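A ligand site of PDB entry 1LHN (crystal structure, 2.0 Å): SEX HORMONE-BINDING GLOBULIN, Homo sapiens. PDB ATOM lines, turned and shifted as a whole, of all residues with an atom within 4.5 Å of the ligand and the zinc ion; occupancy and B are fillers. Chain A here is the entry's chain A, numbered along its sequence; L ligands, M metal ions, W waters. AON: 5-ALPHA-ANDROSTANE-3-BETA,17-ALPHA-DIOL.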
ATOM      1  N   THR A  40       9.408 -17.158  36.043  1.00  0.00           N
ATOM      2  CA  THR A  40       8.533 -16.755  34.954  1.00  0.00           C
ATOM      3  C   THR A  40       8.003 -17.912  34.110  1.00  0.00           C
ATOM      4  O   THR A  40       7.183 -17.710  33.223  1.00  0.00           O
ATOM      5  CB  THR A  40       9.233 -15.766  33.990  1.00  0.00           C
ATOM      6  OG1 THR A  40      10.394 -16.377  33.432  1.00  0.00           O
ATOM      7  CG2 THR A  40       9.624 -14.490  34.722  1.00  0.00           C
ATOM      8  N   SER A  41       8.450 -19.114  34.396  1.00  0.00           N
ATOM      9  CA  SER A  41       8.015 -20.248  33.616  1.00  0.00           C
ATOM     10  C   SER A  41       6.701 -20.902  34.030  1.00  0.00           C
ATOM     11  O   SER A  41       6.238 -20.771  35.171  1.00  0.00           O
ATOM     12  CB  SER A  41       9.104 -21.309  33.612  1.00  0.00           C
ATOM     13  OG  SER A  41       9.114 -22.008  34.845  1.00  0.00           O
ATOM     14  N   SER A  42       6.106 -21.609  33.091  1.00  0.00           N
ATOM     15  CA  SER A  42       4.887 -22.356  33.344  1.00  0.00           C
ATOM     16  C   SER A  42       5.045 -23.695  32.642  1.00  0.00           C
ATOM     17  O   SER A  42       5.669 -23.779  31.576  1.00  0.00           O
ATOM     18  CB  SER A  42       3.655 -21.631  32.820  1.00  0.00           C
ATOM     19  OG  SER A  42       3.428 -20.427  33.536  1.00  0.00           O
ATOM     20  N   PHE A  56      -4.075 -21.939  27.112  1.00  0.00           N
ATOM     21  CA  PHE A  56      -4.071 -20.897  28.120  1.00  0.00           C
ATOM     22  C   PHE A  56      -3.822 -19.515  27.523  1.00  0.00           C
ATOM     23  O   PHE A  56      -3.230 -19.352  26.430  1.00  0.00           O
ATOM     24  CB  PHE A  56      -3.139 -21.231  29.315  1.00  0.00           C
ATOM     25  CG  PHE A  56      -1.714 -20.796  29.141  1.00  0.00           C
ATOM     26  CD1 PHE A  56      -1.324 -19.478  29.392  1.00  0.00           C
ATOM     27  CD2 PHE A  56      -0.741 -21.719  28.756  1.00  0.00           C
ATOM     28  CE1 PHE A  56       0.014 -19.087  29.276  1.00  0.00           C
ATOM     29  CE2 PHE A  56       0.607 -21.337  28.635  1.00  0.00           C
ATOM     30  CZ  PHE A  56       0.979 -20.012  28.897  1.00  0.00           C
ATOM     31  N   GLY A  58      -2.926 -15.293  28.692  1.00  0.00           N
ATOM     32  CA  GLY A  58      -2.284 -14.491  29.714  1.00  0.00           C
ATOM     33  C   GLY A  58      -2.247 -13.049  29.283  1.00  0.00           C
ATOM     34  O   GLY A  58      -2.134 -12.784  28.075  1.00  0.00           O
ATOM     35  N   ASP A  59      -2.372 -12.117  30.231  1.00  0.00           N
ATOM     36  CA  ASP A  59      -2.320 -10.696  29.917  1.00  0.00           C
ATOM     37  C   ASP A  59      -1.948  -9.854  31.125  1.00  0.00           C
ATOM     38  O   ASP A  59      -1.889 -10.356  32.245  1.00  0.00           O
ATOM     39  CB  ASP A  59      -3.641 -10.188  29.314  1.00  0.00           C
ATOM     40  CG  ASP A  59      -4.779 -10.003  30.354  1.00  0.00           C
ATOM     41  OD1 ASP A  59      -4.510  -9.977  31.577  1.00  0.00           O
ATOM     42  OD2 ASP A  59      -5.958  -9.885  29.928  1.00  0.00           O
ATOM     43  N   THR A  60      -1.648  -8.585  30.877  1.00  0.00           N
ATOM     44  CA  THR A  60      -1.357  -7.625  31.932  1.00  0.00           C
ATOM     45  C   THR A  60      -2.345  -6.524  31.593  1.00  0.00           C
ATOM     46  O   THR A  60      -2.601  -5.636  32.407  1.00  0.00           O
ATOM     47  CB  THR A  60       0.067  -7.032  31.838  1.00  0.00           C
ATOM     48  OG1 THR A  60       0.202  -6.251  30.648  1.00  0.00           O
ATOM     49  CG2 THR A  60       1.101  -8.132  31.870  1.00  0.00           C
ATOM     50  N   ASP A  64      -3.917  -4.178  25.123  1.00  0.00           N
ATOM     51  CA  ASP A  64      -2.678  -4.204  24.353  1.00  0.00           C
ATOM     52  C   ASP A  64      -1.478  -4.974  24.909  1.00  0.00           C
ATOM     53  O   ASP A  64      -0.343  -4.723  24.493  1.00  0.00           O
ATOM     54  CB  ASP A  64      -2.241  -2.763  24.121  1.00  0.00           C
ATOM     55  CG  ASP A  64      -2.139  -1.989  25.424  1.00  0.00           C
ATOM     56  OD1 ASP A  64      -1.463  -2.504  26.341  1.00  0.00           O
ATOM     57  OD2 ASP A  64      -2.732  -0.895  25.527  1.00  0.00           O
ATOM     58  N   ASP A  65      -1.727  -5.896  25.835  1.00  0.00           N
ATOM     59  CA  ASP A  65      -0.631  -6.665  26.403  1.00  0.00           C
ATOM     60  C   ASP A  65      -1.114  -8.071  26.699  1.00  0.00           C
ATOM     61  O   ASP A  65      -1.388  -8.411  27.862  1.00  0.00           O
ATOM     62  CB  ASP A  65      -0.176  -6.015  27.716  1.00  0.00           C
ATOM     63  CG  ASP A  65       1.322  -5.976  27.844  1.00  0.00           C
ATOM     64  OD1 ASP A  65       1.913  -4.916  27.554  1.00  0.00           O
ATOM     65  OD2 ASP A  65       1.906  -7.000  28.232  1.00  0.00           O
ATOM     66  N   TRP A  66      -1.209  -8.908  25.677  1.00  0.00           N
ATOM     67  CA  TRP A  66      -1.713 -10.261  25.889  1.00  0.00           C
ATOM     68  C   TRP A  66      -0.983 -11.358  25.128  1.00  0.00           C
ATOM     69  O   TRP A  66      -0.205 -11.108  24.183  1.00  0.00           O
ATOM     70  CB  TRP A  66      -3.218 -10.291  25.603  1.00  0.00           C
ATOM     71  CG  TRP A  66      -3.552  -9.942  24.200  1.00  0.00           C
ATOM     72  CD1 TRP A  66      -3.860  -8.696  23.706  1.00  0.00           C
ATOM     73  CD2 TRP A  66      -3.626 -10.843  23.077  1.00  0.00           C
ATOM     74  NE1 TRP A  66      -4.121  -8.769  22.349  1.00  0.00           N
ATOM     75  CE2 TRP A  66      -3.986 -10.074  21.944  1.00  0.00           C
ATOM     76  CE3 TRP A  66      -3.405 -12.218  22.924  1.00  0.00           C
ATOM     77  CZ2 TRP A  66      -4.145 -10.633  20.675  1.00  0.00           C
ATOM     78  CZ3 TRP A  66      -3.562 -12.786  21.655  1.00  0.00           C
ATOM     79  CH2 TRP A  66      -3.933 -11.988  20.549  1.00  0.00           C
ATOM     80  N   PHE A  67      -1.275 -12.596  25.527  1.00  0.00           N
ATOM     81  CA  PHE A  67      -0.654 -13.802  25.002  1.00  0.00           C
ATOM     82  C   PHE A  67      -1.651 -14.971  24.994  1.00  0.00           C
ATOM     83  O   PHE A  67      -2.499 -15.094  25.888  1.00  0.00           O
ATOM     84  CB  PHE A  67       0.528 -14.155  25.922  1.00  0.00           C
ATOM     85  CG  PHE A  67       1.191 -15.472  25.615  1.00  0.00           C
ATOM     86  CD1 PHE A  67       2.377 -15.507  24.872  1.00  0.00           C
ATOM     87  CD2 PHE A  67       0.694 -16.672  26.153  1.00  0.00           C
ATOM     88  CE1 PHE A  67       3.074 -16.710  24.667  1.00  0.00           C
ATOM     89  CE2 PHE A  67       1.371 -17.888  25.952  1.00  0.00           C
ATOM     90  CZ  PHE A  67       2.569 -17.910  25.211  1.00  0.00           C
ATOM     91  N   LEU A  80       0.573 -13.362  20.205  1.00  0.00           N
ATOM     92  CA  LEU A  80       1.149 -12.463  21.193  1.00  0.00           C
ATOM     93  C   LEU A  80       0.959 -11.049  20.705  1.00  0.00           C
ATOM     94  O   LEU A  80       1.127 -10.773  19.506  1.00  0.00           O
ATOM     95  CB  LEU A  80       2.648 -12.833  21.304  1.00  0.00           C
ATOM     96  CG  LEU A  80       3.748 -12.187  22.117  1.00  0.00           C
ATOM     97  CD1 LEU A  80       4.842 -13.254  22.336  1.00  0.00           C
ATOM     98  CD2 LEU A  80       4.296 -10.949  21.386  1.00  0.00           C
ATOM     99  N   ASN A  82       1.956  -7.146  22.178  1.00  0.00           N
ATOM    100  CA  ASN A  82       2.448  -6.201  23.180  1.00  0.00           C
ATOM    101  C   ASN A  82       3.179  -5.045  22.508  1.00  0.00           C
ATOM    102  O   ASN A  82       3.196  -4.934  21.276  1.00  0.00           O
ATOM    103  CB  ASN A  82       3.325  -6.881  24.248  1.00  0.00           C
ATOM    104  CG  ASN A  82       4.669  -7.351  23.729  1.00  0.00           C
ATOM    105  OD1 ASN A  82       5.162  -6.898  22.698  1.00  0.00           O
ATOM    106  ND2 ASN A  82       5.304  -8.252  24.479  1.00  0.00           N
ATOM    107  N   HIS A  83       3.774  -4.174  23.314  1.00  0.00           N
ATOM    108  CA  HIS A  83       4.482  -3.014  22.782  1.00  0.00           C
ATOM    109  C   HIS A  83       5.609  -3.352  21.781  1.00  0.00           C
ATOM    110  O   HIS A  83       5.850  -2.596  20.844  1.00  0.00           O
ATOM    111  CB  HIS A  83       5.063  -2.194  23.945  1.00  0.00           C
ATOM    112  CG  HIS A  83       4.024  -1.669  24.883  1.00  0.00           C
ATOM    113  ND1 HIS A  83       3.088  -0.723  24.513  1.00  0.00           N
ATOM    114  CD2 HIS A  83       3.773  -1.945  26.191  1.00  0.00           C
ATOM    115  CE1 HIS A  83       2.305  -0.447  25.542  1.00  0.00           C
ATOM    116  NE2 HIS A  83       2.695  -1.175  26.570  1.00  0.00           N
ATOM    117  N   VAL A 105       6.490 -23.197  28.924  1.00  0.00           N
ATOM    118  CA  VAL A 105       6.545 -21.873  28.341  1.00  0.00           C
ATOM    119  C   VAL A 105       7.353 -21.012  29.295  1.00  0.00           C
ATOM    120  O   VAL A 105       7.023 -20.891  30.493  1.00  0.00           O
ATOM    121  CB  VAL A 105       5.155 -21.252  28.139  1.00  0.00           C
ATOM    122  CG1 VAL A 105       5.303 -19.886  27.456  1.00  0.00           C
ATOM    123  CG2 VAL A 105       4.290 -22.182  27.264  1.00  0.00           C
ATOM    124  N   LYS A 106       8.400 -20.406  28.783  1.00  0.00           N
ATOM    125  CA  LYS A 106       9.237 -19.625  29.658  1.00  0.00           C
ATOM    126  C   LYS A 106       9.876 -18.425  29.007  1.00  0.00           C
ATOM    127  O   LYS A 106       9.942 -18.313  27.789  1.00  0.00           O
ATOM    128  CB  LYS A 106      10.341 -20.536  30.225  1.00  0.00           C
ATOM    129  CG  LYS A 106      11.100 -21.249  29.127  1.00  0.00           C
ATOM    130  CD  LYS A 106      12.248 -22.146  29.621  1.00  0.00           C
ATOM    131  CE  LYS A 106      11.774 -23.460  30.216  1.00  0.00           C
ATOM    132  NZ  LYS A 106      11.109 -23.306  31.546  1.00  0.00           N
ATOM    133  N   MET A 107      10.339 -17.515  29.862  1.00  0.00           N
ATOM    134  CA  MET A 107      11.014 -16.327  29.410  1.00  0.00           C
ATOM    135  C   MET A 107      12.511 -16.606  29.504  1.00  0.00           C
ATOM    136  O   MET A 107      12.972 -17.212  30.469  1.00  0.00           O
ATOM    137  CB  MET A 107      10.663 -15.146  30.308  1.00  0.00           C
ATOM    138  CG  MET A 107       9.229 -14.702  30.197  1.00  0.00           C
ATOM    139  SD  MET A 107       8.814 -14.328  28.473  1.00  0.00           S
ATOM    140  CE  MET A 107      10.105 -13.116  28.075  1.00  0.00           C
ATOM    141  N   VAL A 112      10.508 -15.653  24.361  1.00  0.00           N
ATOM    142  CA  VAL A 112       9.495 -16.556  24.909  1.00  0.00           C
ATOM    143  C   VAL A 112       9.827 -17.888  24.256  1.00  0.00           C
ATOM    144  O   VAL A 112       9.899 -18.010  23.032  1.00  0.00           O
ATOM    145  CB  VAL A 112       8.062 -16.115  24.562  1.00  0.00           C
ATOM    146  CG1 VAL A 112       7.046 -17.211  24.965  1.00  0.00           C
ATOM    147  CG2 VAL A 112       7.731 -14.840  25.288  1.00  0.00           C
ATOM    148  N   SER A 128       9.727  -9.196  24.432  1.00  0.00           N
ATOM    149  CA  SER A 128       9.345  -8.601  25.707  1.00  0.00           C
ATOM    150  C   SER A 128      10.488  -8.038  26.544  1.00  0.00           C
ATOM    151  O   SER A 128      11.617  -8.502  26.478  1.00  0.00           O
ATOM    152  CB  SER A 128       8.588  -9.640  26.536  1.00  0.00           C
ATOM    153  OG  SER A 128       8.268  -9.145  27.824  1.00  0.00           O
ATOM    154  N   LEU A 131       9.359  -8.530  32.840  1.00  0.00           N
ATOM    155  CA  LEU A 131       7.974  -8.571  33.318  1.00  0.00           C
ATOM    156  C   LEU A 131       7.832  -7.706  34.566  1.00  0.00           C
ATOM    157  O   LEU A 131       7.052  -6.736  34.578  1.00  0.00           O
ATOM    158  CB  LEU A 131       7.535  -9.997  33.635  1.00  0.00           C
ATOM    159  CG  LEU A 131       7.087 -10.902  32.481  1.00  0.00           C
ATOM    160  CD1 LEU A 131       6.688 -12.264  33.032  1.00  0.00           C
ATOM    161  CD2 LEU A 131       5.918 -10.259  31.755  1.00  0.00           C
ATOM    162  N   HIS A 136       1.586  -2.265  34.220  1.00  0.00           N
ATOM    163  CA  HIS A 136       1.369  -3.704  34.107  1.00  0.00           C
ATOM    164  C   HIS A 136       1.827  -4.382  35.388  1.00  0.00           C
ATOM    165  O   HIS A 136       2.636  -5.306  35.357  1.00  0.00           O
ATOM    166  CB  HIS A 136       2.166  -4.292  32.933  1.00  0.00           C
ATOM    167  CG  HIS A 136       2.553  -3.288  31.889  1.00  0.00           C
ATOM    168  ND1 HIS A 136       3.439  -2.250  32.141  1.00  0.00           N
ATOM    169  CD2 HIS A 136       2.192  -3.164  30.590  1.00  0.00           C
ATOM    170  CE1 HIS A 136       3.596  -1.531  31.034  1.00  0.00           C
ATOM    171  NE2 HIS A 136       2.857  -2.062  30.089  1.00  0.00           N
ATOM    172  N   MET A 139      -0.561  -9.639  36.322  1.00  0.00           N
ATOM    173  CA  MET A 139      -0.683 -10.590  35.207  1.00  0.00           C
ATOM    174  C   MET A 139      -1.800 -11.589  35.512  1.00  0.00           C
ATOM    175  O   MET A 139      -1.875 -12.139  36.612  1.00  0.00           O
ATOM    176  CB  MET A 139       0.612 -11.377  35.012  1.00  0.00           C
ATOM    177  CG  MET A 139       0.520 -12.443  33.898  1.00  0.00           C
ATOM    178  SD  MET A 139       2.130 -13.178  33.529  1.00  0.00           S
ATOM    179  CE  MET A 139       2.926 -11.756  32.832  1.00  0.00           C
ATOM    180  N   ILE A 141      -3.688 -15.207  34.234  1.00  0.00           N
ATOM    181  CA  ILE A 141      -3.519 -16.437  33.452  1.00  0.00           C
ATOM    182  C   ILE A 141      -4.883 -17.147  33.451  1.00  0.00           C
ATOM    183  O   ILE A 141      -5.422 -17.443  34.521  1.00  0.00           O
ATOM    184  CB  ILE A 141      -2.493 -17.432  34.066  1.00  0.00           C
ATOM    185  CG1 ILE A 141      -1.081 -16.843  34.106  1.00  0.00           C
ATOM    186  CG2 ILE A 141      -2.482 -18.737  33.226  1.00  0.00           C
ATOM    187  CD1 ILE A 141      -0.469 -16.528  32.768  1.00  0.00           C
ATOM    188  N   LEU A 171       3.813 -19.794  36.635  1.00  0.00           N
ATOM    189  CA  LEU A 171       4.679 -18.715  37.105  1.00  0.00           C
ATOM    190  C   LEU A 171       5.205 -18.974  38.513  1.00  0.00           C
ATOM    191  O   LEU A 171       5.736 -20.034  38.822  1.00  0.00           O
ATOM    192  CB  LEU A 171       3.920 -17.396  37.082  1.00  0.00           C
ATOM    193  CG  LEU A 171       3.565 -16.835  35.713  1.00  0.00           C
ATOM    194  CD1 LEU A 171       2.280 -16.013  35.793  1.00  0.00           C
ATOM    195  CD2 LEU A 171       4.732 -16.002  35.206  1.00  0.00           C
HETATM  196  C1  AON L   1       5.771 -15.590  30.051  1.00  0.00           C
HETATM  197  C10 AON L   1       4.364 -15.263  29.447  1.00  0.00           C
HETATM  198  C11 AON L   1       5.303 -13.129  28.227  1.00  0.00           C
HETATM  199  C12 AON L   1       5.132 -11.583  28.011  1.00  0.00           C
HETATM  200  C13 AON L   1       3.732 -11.251  27.451  1.00  0.00           C
HETATM  201  C14 AON L   1       2.656 -11.801  28.458  1.00  0.00           C
HETATM  202  C15 AON L   1       1.320 -11.188  27.957  1.00  0.00           C
HETATM  203  C16 AON L   1       1.774  -9.819  27.328  1.00  0.00           C
HETATM  204  C17 AON L   1       3.311  -9.771  27.476  1.00  0.00           C
HETATM  205  C18 AON L   1       3.605 -11.795  25.993  1.00  0.00           C
HETATM  206  C19 AON L   1       4.234 -16.026  28.074  1.00  0.00           C
HETATM  207  C2  AON L   1       5.930 -17.110  30.408  1.00  0.00           C
HETATM  208  C3  AON L   1       4.795 -17.520  31.380  1.00  0.00           C
HETATM  209  C4  AON L   1       3.387 -17.243  30.798  1.00  0.00           C
HETATM  210  C5  AON L   1       3.245 -15.728  30.480  1.00  0.00           C
HETATM  211  C6  AON L   1       1.841 -15.407  29.912  1.00  0.00           C
HETATM  212  C7  AON L   1       1.696 -13.880  29.643  1.00  0.00           C
HETATM  213  C8  AON L   1       2.777 -13.338  28.659  1.00  0.00           C
HETATM  214  C9  AON L   1       4.215 -13.694  29.197  1.00  0.00           C
HETATM  215  O3  AON L   1       4.940 -18.922  31.710  1.00  0.00           O
HETATM  216  O17 AON L   1       3.651  -9.054  28.733  1.00  0.00           O
HETATM  217 ZN    ZN M   1       1.694  -2.473  28.299  1.00  0.00          ZN
HETATM  218  O   HOH W   1       5.973  -8.402  28.034  1.00  0.00           O
HETATM  219  O   HOH W   2       1.867   0.507  29.877  1.00  0.00           O
HETATM  220  O   HOH W   3       0.057  -1.188  28.239  1.00  0.00           O
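OD1 of Asp 64 touches the zinc ion, at 3.7 Å.
Of the 24 residues printed, 4 come within 4 Å of the zinc ion.
The nearest printed residue that does not touch the zinc ion is Thr 60 (4.7 Å).
O of Asp 65 is in hydrogen-bond range of N of Thr 60 (3.0 Å).
O of Ser 42 lies within hydrogen-bond range of N of Val 105 (2.8 Å).
The side-chain hydroxyl (OG) of Ser 42 lies within hydrogen-bond range of the backbone NH (N) of Leu 171, 3.2 Å away.
The backbone NH (N) of Leu 171 sits at hydrogen-bond distance from the backbone carbonyl oxygen (O) of Ser 41 (3.0 Å).
N of Phe 67 is in hydrogen-bond range of O of Gly 58 (2.7 Å).
The zinc ion is bound by water W3 (2.1 Å), NE2 of His 136 (2.2 Å), NE2 of His 83 (2.4 Å) and OD1 of Asp 65 (2.6 Å).
The zinc ion has four donor atoms within binding distance.
An oxygen (O17) of the ligand sits at hydrogen-bond distance from the side-chain carboxylate (OD2) of Asp 65, 2.7 Å away.
An oxygen (O3) of the ligand sits close to the backbone NH (N) of Ser 42, at 3.2 Å.
The side-chain hydroxyl (OG) of Ser 42 sits at hydrogen-bond distance from an oxygen (O3) of the ligand (2.8 Å).
The backbone carbonyl oxygen of Thr 40 lies within hydrogen-bond range of an oxygen (O3) of the ligand (3.0 Å).
O of Val 105 is in hydrogen-bond range of O3 of the ligand, at 3.1 Å.
Water W1 lies within hydrogen-bond range of the side-chain hydroxyl of Ser 128 (2.4 Å) and an oxygen (O17) of the ligand (2.5 Å).
Residues that only touch the ligand: Ser 41, Gly 58, Trp 66, Phe 67, Leu 80, Asn 82, Met 107, Ser 128, Leu 131, Met 139 and Ile 141.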
